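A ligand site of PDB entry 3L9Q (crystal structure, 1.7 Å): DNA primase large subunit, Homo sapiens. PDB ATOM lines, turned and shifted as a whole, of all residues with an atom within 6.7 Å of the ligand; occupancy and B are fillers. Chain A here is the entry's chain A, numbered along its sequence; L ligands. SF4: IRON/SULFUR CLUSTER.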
ATOM      1  N   PRO A  16      21.625  21.237 -18.433  1.00  0.00           N
ATOM      2  CA  PRO A  16      22.782  20.379 -18.686  1.00  0.00           C
ATOM      3  C   PRO A  16      22.315  19.023 -19.235  1.00  0.00           C
ATOM      4  O   PRO A  16      21.130  18.703 -19.111  1.00  0.00           O
ATOM      5  CB  PRO A  16      23.416  20.207 -17.300  1.00  0.00           C
ATOM      6  CG  PRO A  16      22.371  20.569 -16.306  1.00  0.00           C
ATOM      7  CD  PRO A  16      21.346  21.440 -16.996  1.00  0.00           C
ATOM      8  N   PRO A  17      23.221  18.244 -19.846  1.00  0.00           N
ATOM      9  CA  PRO A  17      22.806  16.989 -20.478  1.00  0.00           C
ATOM     10  C   PRO A  17      22.005  16.050 -19.565  1.00  0.00           C
ATOM     11  O   PRO A  17      21.084  15.369 -20.041  1.00  0.00           O
ATOM     12  CB  PRO A  17      24.144  16.365 -20.908  1.00  0.00           C
ATOM     13  CG  PRO A  17      25.009  17.568 -21.181  1.00  0.00           C
ATOM     14  CD  PRO A  17      24.655  18.530 -20.086  1.00  0.00           C
ATOM     15  N   CYS A  18      22.343  16.000 -18.279  1.00  0.00           N
ATOM     16  CA  CYS A  18      21.624  15.109 -17.359  1.00  0.00           C
ATOM     17  C   CYS A  18      20.145  15.443 -17.250  1.00  0.00           C
ATOM     18  O   CYS A  18      19.300  14.547 -17.158  1.00  0.00           O
ATOM     19  CB  CYS A  18      22.274  15.122 -15.970  1.00  0.00           C
ATOM     20  SG  CYS A  18      22.363  16.785 -15.226  1.00  0.00           S
ATOM     21  N   MET A  19      19.810  16.738 -17.267  1.00  0.00           N
ATOM     22  CA  MET A  19      18.423  17.156 -17.122  1.00  0.00           C
ATOM     23  C   MET A  19      17.739  17.235 -18.482  1.00  0.00           C
ATOM     24  O   MET A  19      16.531  16.981 -18.614  1.00  0.00           O
ATOM     25  CB  MET A  19      18.340  18.504 -16.419  1.00  0.00           C
ATOM     26  CG  MET A  19      19.045  18.497 -15.058  1.00  0.00           C
ATOM     27  SD  MET A  19      18.370  17.239 -13.929  1.00  0.00           S
ATOM     28  CE  MET A  19      19.485  17.498 -12.534  1.00  0.00           C
ATOM     29  N   GLN A  39      15.548  13.273  -9.641  1.00  0.00           N
ATOM     30  CA  GLN A  39      16.617  14.096 -10.212  1.00  0.00           C
ATOM     31  C   GLN A  39      16.070  15.294 -10.990  1.00  0.00           C
ATOM     32  O   GLN A  39      16.492  16.435 -10.767  1.00  0.00           O
ATOM     33  CB  GLN A  39      17.533  13.254 -11.100  1.00  0.00           C
ATOM     34  CG  GLN A  39      18.648  14.048 -11.735  1.00  0.00           C
ATOM     35  CD  GLN A  39      19.651  13.165 -12.458  1.00  0.00           C
ATOM     36  OE1 GLN A  39      19.964  12.060 -12.024  1.00  0.00           O
ATOM     37  NE2 GLN A  39      20.163  13.666 -13.578  1.00  0.00           N
ATOM     38  N   SER A  97      23.482  17.548  -6.509  1.00  0.00           N
ATOM     39  CA  SER A  97      24.730  18.075  -7.058  1.00  0.00           C
ATOM     40  C   SER A  97      25.295  17.126  -8.119  1.00  0.00           C
ATOM     41  O   SER A  97      24.813  15.995  -8.268  1.00  0.00           O
ATOM     42  CB  SER A  97      25.769  18.215  -5.937  1.00  0.00           C
ATOM     43  OG  SER A  97      26.119  16.923  -5.453  1.00  0.00           O
ATOM     44  N   CYS A  98      26.302  17.577  -8.850  1.00  0.00           N
ATOM     45  CA  CYS A  98      26.963  16.702  -9.827  1.00  0.00           C
ATOM     46  C   CYS A  98      27.529  15.458  -9.152  1.00  0.00           C
ATOM     47  O   CYS A  98      27.390  14.353  -9.672  1.00  0.00           O
ATOM     48  CB  CYS A  98      28.078  17.451 -10.571  1.00  0.00           C
ATOM     49  SG  CYS A  98      27.505  18.760 -11.684  1.00  0.00           S
ATOM     50  N   LEU A  99      28.186  15.640  -8.012  1.00  0.00           N
ATOM     51  CA  LEU A  99      28.792  14.488  -7.333  1.00  0.00           C
ATOM     52  C   LEU A  99      27.740  13.491  -6.887  1.00  0.00           C
ATOM     53  O   LEU A  99      27.933  12.285  -6.980  1.00  0.00           O
ATOM     54  CB  LEU A  99      29.669  14.938  -6.166  1.00  0.00           C
ATOM     55  CG  LEU A  99      31.007  15.522  -6.618  1.00  0.00           C
ATOM     56  CD1 LEU A  99      31.870  15.860  -5.406  1.00  0.00           C
ATOM     57  CD2 LEU A  99      31.732  14.543  -7.534  1.00  0.00           C
ATOM     58  N   ILE A 101      24.842  12.976  -8.336  1.00  0.00           N
ATOM     59  CA  ILE A 101      24.360  12.312  -9.551  1.00  0.00           C
ATOM     60  C   ILE A 101      25.387  11.312 -10.104  1.00  0.00           C
ATOM     61  O   ILE A 101      25.044  10.185 -10.509  1.00  0.00           O
ATOM     62  CB  ILE A 101      23.982  13.347 -10.630  1.00  0.00           C
ATOM     63  CG1 ILE A 101      22.795  14.197 -10.155  1.00  0.00           C
ATOM     64  CG2 ILE A 101      23.673  12.666 -11.961  1.00  0.00           C
ATOM     65  CD1 ILE A 101      22.495  15.429 -11.023  1.00  0.00           C
ATOM     66  N   ILE A 102      26.654  11.715 -10.107  1.00  0.00           N
ATOM     67  CA  ILE A 102      27.737  10.903 -10.675  1.00  0.00           C
ATOM     68  C   ILE A 102      28.050   9.679  -9.815  1.00  0.00           C
ATOM     69  O   ILE A 102      28.264   8.589 -10.336  1.00  0.00           O
ATOM     70  CB  ILE A 102      28.998  11.759 -10.907  1.00  0.00           C
ATOM     71  CG1 ILE A 102      28.753  12.722 -12.081  1.00  0.00           C
ATOM     72  CG2 ILE A 102      30.229  10.875 -11.158  1.00  0.00           C
ATOM     73  CD1 ILE A 102      29.729  13.884 -12.136  1.00  0.00           C
ATOM     74  N   GLY A 114      20.865  10.025 -13.957  1.00  0.00           N
ATOM     75  CA  GLY A 114      22.310   9.919 -13.929  1.00  0.00           C
ATOM     76  C   GLY A 114      22.975  11.046 -14.687  1.00  0.00           C
ATOM     77  O   GLY A 114      22.326  12.049 -15.047  1.00  0.00           O
ATOM     78  N   CYS A 115      24.272  10.903 -14.915  1.00  0.00           N
ATOM     79  CA  CYS A 115      25.063  11.870 -15.662  1.00  0.00           C
ATOM     80  C   CYS A 115      25.539  11.180 -16.922  1.00  0.00           C
ATOM     81  O   CYS A 115      26.272  10.181 -16.839  1.00  0.00           O
ATOM     82  CB  CYS A 115      26.276  12.289 -14.843  1.00  0.00           C
ATOM     83  SG  CYS A 115      27.477  13.279 -15.769  1.00  0.00           S
ATOM     84  N   PRO A 116      25.151  11.701 -18.094  1.00  0.00           N
ATOM     85  CA  PRO A 116      25.495  10.982 -19.342  1.00  0.00           C
ATOM     86  C   PRO A 116      27.007  10.825 -19.517  1.00  0.00           C
ATOM     87  O   PRO A 116      27.464   9.830 -20.090  1.00  0.00           O
ATOM     88  CB  PRO A 116      24.936  11.881 -20.444  1.00  0.00           C
ATOM     89  CG  PRO A 116      23.996  12.828 -19.779  1.00  0.00           C
ATOM     90  CD  PRO A 116      24.370  12.924 -18.340  1.00  0.00           C
ATOM     91  N   PHE A 117      27.787  11.792 -19.046  1.00  0.00           N
ATOM     92  CA  PHE A 117      29.230  11.704 -19.210  1.00  0.00           C
ATOM     93  C   PHE A 117      29.794  10.528 -18.421  1.00  0.00           C
ATOM     94  O   PHE A 117      30.740   9.868 -18.860  1.00  0.00           O
ATOM     95  CB  PHE A 117      29.886  13.031 -18.824  1.00  0.00           C
ATOM     96  CG  PHE A 117      29.421  14.182 -19.647  1.00  0.00           C
ATOM     97  CD1 PHE A 117      29.816  14.304 -20.979  1.00  0.00           C
ATOM     98  CD2 PHE A 117      28.583  15.144 -19.111  1.00  0.00           C
ATOM     99  CE1 PHE A 117      29.386  15.361 -21.753  1.00  0.00           C
ATOM    100  CE2 PHE A 117      28.142  16.213 -19.882  1.00  0.00           C
ATOM    101  CZ  PHE A 117      28.542  16.327 -21.199  1.00  0.00           C
ATOM    102  N   ARG A 118      29.174  10.256 -17.279  1.00  0.00           N
ATOM    103  CA  ARG A 118      29.583   9.164 -16.394  1.00  0.00           C
ATOM    104  C   ARG A 118      28.915   7.835 -16.751  1.00  0.00           C
ATOM    105  O   ARG A 118      29.567   6.779 -16.761  1.00  0.00           O
ATOM    106  CB  ARG A 118      29.254   9.548 -14.944  1.00  0.00           C
ATOM    107  CG  ARG A 118      29.157   8.374 -13.990  1.00  0.00           C
ATOM    108  CD  ARG A 118      30.508   7.700 -13.775  1.00  0.00           C
ATOM    109  NE  ARG A 118      30.400   6.599 -12.821  1.00  0.00           N
ATOM    110  CZ  ARG A 118      29.979   5.380 -13.156  1.00  0.00           C
ATOM    111  NH1 ARG A 118      29.646   5.108 -14.414  1.00  0.00           N
ATOM    112  NH2 ARG A 118      29.890   4.425 -12.232  1.00  0.00           N
ATOM    113  N   TYR A 151      34.300  14.124 -15.809  1.00  0.00           N
ATOM    114  CA  TYR A 151      32.920  14.273 -16.264  1.00  0.00           C
ATOM    115  C   TYR A 151      32.446  15.722 -16.231  1.00  0.00           C
ATOM    116  O   TYR A 151      31.889  16.217 -17.208  1.00  0.00           O
ATOM    117  CB  TYR A 151      31.993  13.373 -15.444  1.00  0.00           C
ATOM    118  CG  TYR A 151      32.496  11.963 -15.388  1.00  0.00           C
ATOM    119  CD1 TYR A 151      32.703  11.250 -16.558  1.00  0.00           C
ATOM    120  CD2 TYR A 151      32.807  11.352 -14.178  1.00  0.00           C
ATOM    121  CE1 TYR A 151      33.186   9.946 -16.537  1.00  0.00           C
ATOM    122  CE2 TYR A 151      33.296  10.051 -14.145  1.00  0.00           C
ATOM    123  CZ  TYR A 151      33.476   9.357 -15.330  1.00  0.00           C
ATOM    124  OH  TYR A 151      33.957   8.075 -15.304  1.00  0.00           O
ATOM    125  N   GLN A 152      32.687  16.401 -15.112  1.00  0.00           N
ATOM    126  CA  GLN A 152      32.239  17.780 -14.974  1.00  0.00           C
ATOM    127  C   GLN A 152      32.990  18.730 -15.897  1.00  0.00           C
ATOM    128  O   GLN A 152      32.425  19.706 -16.394  1.00  0.00           O
ATOM    129  CB  GLN A 152      32.340  18.220 -13.507  1.00  0.00           C
ATOM    130  CG  GLN A 152      31.373  17.470 -12.585  1.00  0.00           C
ATOM    131  CD  GLN A 152      31.868  17.422 -11.151  1.00  0.00           C
ATOM    132  OE1 GLN A 152      32.376  16.399 -10.698  1.00  0.00           O
ATOM    133  NE2 GLN A 152      31.732  18.528 -10.440  1.00  0.00           N
ATOM    134  N   VAL A 153      34.267  18.449 -16.152  1.00  0.00           N
ATOM    135  CA  VAL A 153      35.018  19.244 -17.124  1.00  0.00           C
ATOM    136  C   VAL A 153      34.526  18.984 -18.555  1.00  0.00           C
ATOM    137  O   VAL A 153      34.499  19.900 -19.370  1.00  0.00           O
ATOM    138  CB  VAL A 153      36.535  19.017 -16.971  1.00  0.00           C
ATOM    139  CG1 VAL A 153      37.300  19.837 -18.009  1.00  0.00           C
ATOM    140  CG2 VAL A 153      36.961  19.419 -15.568  1.00  0.00           C
ATOM    141  N   ALA A 154      34.117  17.746 -18.836  1.00  0.00           N
ATOM    142  CA  ALA A 154      33.472  17.448 -20.118  1.00  0.00           C
ATOM    143  C   ALA A 154      32.172  18.251 -20.247  1.00  0.00           C
ATOM    144  O   ALA A 154      31.845  18.759 -21.326  1.00  0.00           O
ATOM    145  CB  ALA A 154      33.171  15.950 -20.248  1.00  0.00           C
ATOM    146  N   CYS A 155      31.434  18.358 -19.147  1.00  0.00           N
ATOM    147  CA  CYS A 155      30.178  19.090 -19.164  1.00  0.00           C
ATOM    148  C   CYS A 155      30.433  20.590 -19.361  1.00  0.00           C
ATOM    149  O   CYS A 155      29.652  21.279 -20.010  1.00  0.00           O
ATOM    150  CB  CYS A 155      29.397  18.831 -17.878  1.00  0.00           C
ATOM    151  SG  CYS A 155      27.715  19.423 -17.923  1.00  0.00           S
ATOM    152  N   GLN A 156      31.530  21.091 -18.805  1.00  0.00           N
ATOM    153  CA  GLN A 156      31.919  22.480 -19.042  1.00  0.00           C
ATOM    154  C   GLN A 156      32.229  22.707 -20.522  1.00  0.00           C
ATOM    155  O   GLN A 156      31.880  23.745 -21.084  1.00  0.00           O
ATOM    156  CB  GLN A 156      33.144  22.853 -18.196  1.00  0.00           C
ATOM    157  CG  GLN A 156      32.847  22.965 -16.710  1.00  0.00           C
ATOM    158  CD  GLN A 156      34.095  23.218 -15.890  1.00  0.00           C
ATOM    159  OE1 GLN A 156      35.180  23.492 -16.426  1.00  0.00           O
ATOM    160  NE2 GLN A 156      33.955  23.104 -14.583  1.00  0.00           N
ATOM    161  N   LEU A 172      32.250  23.874 -12.537  1.00  0.00           N
ATOM    162  CA  LEU A 172      30.945  23.225 -12.452  1.00  0.00           C
ATOM    163  C   LEU A 172      30.864  22.203 -11.321  1.00  0.00           C
ATOM    164  O   LEU A 172      31.691  21.290 -11.235  1.00  0.00           O
ATOM    165  CB  LEU A 172      30.611  22.516 -13.775  1.00  0.00           C
ATOM    166  CG  LEU A 172      29.285  21.758 -13.770  1.00  0.00           C
ATOM    167  CD1 LEU A 172      28.087  22.718 -13.668  1.00  0.00           C
ATOM    168  CD2 LEU A 172      29.182  20.895 -15.019  1.00  0.00           C
ATOM    169  N   ASN A 173      29.846  22.345 -10.470  1.00  0.00           N
ATOM    170  CA  ASN A 173      29.620  21.379  -9.408  1.00  0.00           C
ATOM    171  C   ASN A 173      28.144  21.058  -9.197  1.00  0.00           C
ATOM    172  O   ASN A 173      27.816  20.225  -8.351  1.00  0.00           O
ATOM    173  CB  ASN A 173      30.273  21.846  -8.100  1.00  0.00           C
ATOM    174  CG  ASN A 173      29.739  23.185  -7.621  1.00  0.00           C
ATOM    175  OD1 ASN A 173      28.528  23.379  -7.506  1.00  0.00           O
ATOM    176  ND2 ASN A 173      30.635  24.121  -7.341  1.00  0.00           N
ATOM    177  N   HIS A 174      27.258  21.697  -9.962  1.00  0.00           N
ATOM    178  CA  HIS A 174      25.812  21.508  -9.751  1.00  0.00           C
ATOM    179  C   HIS A 174      25.002  21.792 -11.013  1.00  0.00           C
ATOM    180  O   HIS A 174      25.190  22.823 -11.666  1.00  0.00           O
ATOM    181  CB  HIS A 174      25.351  22.444  -8.625  1.00  0.00           C
ATOM    182  CG  HIS A 174      24.120  21.967  -7.896  1.00  0.00           C
ATOM    183  ND1 HIS A 174      22.855  22.002  -8.454  1.00  0.00           N
ATOM    184  CD2 HIS A 174      23.964  21.482  -6.643  1.00  0.00           C
ATOM    185  CE1 HIS A 174      21.977  21.542  -7.583  1.00  0.00           C
ATOM    186  NE2 HIS A 174      22.624  21.212  -6.481  1.00  0.00           N
ATOM    187  N   PRO A 175      24.080  20.883 -11.365  1.00  0.00           N
ATOM    188  CA  PRO A 175      23.209  21.144 -12.523  1.00  0.00           C
ATOM    189  C   PRO A 175      22.503  22.499 -12.434  1.00  0.00           C
ATOM    190  O   PRO A 175      22.345  23.172 -13.457  1.00  0.00           O
ATOM    191  CB  PRO A 175      22.180  20.002 -12.439  1.00  0.00           C
ATOM    192  CG  PRO A 175      22.918  18.878 -11.772  1.00  0.00           C
ATOM    193  CD  PRO A 175      23.801  19.574 -10.743  1.00  0.00           C
ATOM    194  N   ASN A 176      22.069  22.892 -11.247  1.00  0.00           N
ATOM    195  CA  ASN A 176      21.374  24.177 -11.102  1.00  0.00           C
ATOM    196  C   ASN A 176      22.318  25.381 -11.300  1.00  0.00           C
ATOM    197  O   ASN A 176      21.885  26.479 -11.669  1.00  0.00           O
ATOM    198  CB  ASN A 176      20.646  24.253  -9.771  1.00  0.00           C
ATOM    199  CG  ASN A 176      19.387  23.406  -9.773  1.00  0.00           C
ATOM    200  OD1 ASN A 176      19.408  22.252  -9.328  1.00  0.00           O
ATOM    201  ND2 ASN A 176      18.293  23.950 -10.296  1.00  0.00           N
ATOM    202  N   PHE A 178      24.879  25.184 -13.540  1.00  0.00           N
ATOM    203  CA  PHE A 178      24.897  25.159 -15.001  1.00  0.00           C
ATOM    204  C   PHE A 178      23.736  25.988 -15.557  1.00  0.00           C
ATOM    205  O   PHE A 178      23.937  26.834 -16.432  1.00  0.00           O
ATOM    206  CB  PHE A 178      24.802  23.709 -15.483  1.00  0.00           C
ATOM    207  CG  PHE A 178      24.943  23.534 -16.980  1.00  0.00           C
ATOM    208  CD1 PHE A 178      26.038  22.855 -17.500  1.00  0.00           C
ATOM    209  CD2 PHE A 178      23.969  24.002 -17.845  1.00  0.00           C
ATOM    210  CE1 PHE A 178      26.175  22.657 -18.872  1.00  0.00           C
ATOM    211  CE2 PHE A 178      24.098  23.823 -19.225  1.00  0.00           C
ATOM    212  CZ  PHE A 178      25.198  23.137 -19.730  1.00  0.00           C
HETATM  213 FE1  SF4 L   1      26.811  18.044 -16.267  1.00  0.00          FE
HETATM  214 FE2  SF4 L   1      26.847  15.495 -15.352  1.00  0.00          FE
HETATM  215 FE3  SF4 L   1      26.870  17.583 -13.575  1.00  0.00          FE
HETATM  216 FE4  SF4 L   1      24.633  17.016 -15.045  1.00  0.00          FE
HETATM  217  S1  SF4 L   1      25.611  15.692 -13.421  1.00  0.00           S
HETATM  218  S2  SF4 L   1      25.513  19.091 -14.686  1.00  0.00           S
HETATM  219  S3  SF4 L   1      25.530  16.342 -17.050  1.00  0.00           S
HETATM  220  S4  SF4 L   1      28.517  17.021 -15.081  1.00  0.00           S
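Residues that only touch the ligand: Pro 16, Pro 175, Gln 152, Pro 116, Pro 17, Phe 117, Ile 101 and Leu 172.
Hydrophobic or aromatic side chains within 4 Å of the ligand: Pro 16, Pro 17, Ile 101, Pro 116, Phe 117, Leu 172 and Pro 175.
The nearest printed residue that does not touch the ligand is Tyr 151 (4.1 Å).
NE2 of Gln 152 sits at hydrogen-bond distance from O of Leu 172 (2.9 Å).
The backbone NH of Cys 98 is in hydrogen-bond range of the backbone carbonyl oxygen of Asn 173 (3.1 Å).
The backbone NH of His 174 lies close to the side-chain sulfur of Cys 98 (3.4 Å).
The backbone NH of Leu 172 sits close to the side-chain amide nitrogen of Gln 156 (2.8 Å).
SG of Cys 115 sits close to N of Arg 118 (3.8 Å).
SG of Cys 115 sits close to N of Phe 117 (3.6 Å).
The backbone NH of Cys 18 sits close to a sulfur (S3) of the ligand, 3.4 Å away.
FE2 of the ligand is bound by SG of Cys 115 (2.3 Å).
The side-chain sulfur of Cys 18 binds an iron atom (FE4) of the ligand, at 2.3 Å.
An iron atom (FE3) of the ligand is bound by the side-chain sulfur (SG) of Cys 98 (2.3 Å).
SG of Cys 155 is bound to FE1 of the ligand, at 2.3 Å.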
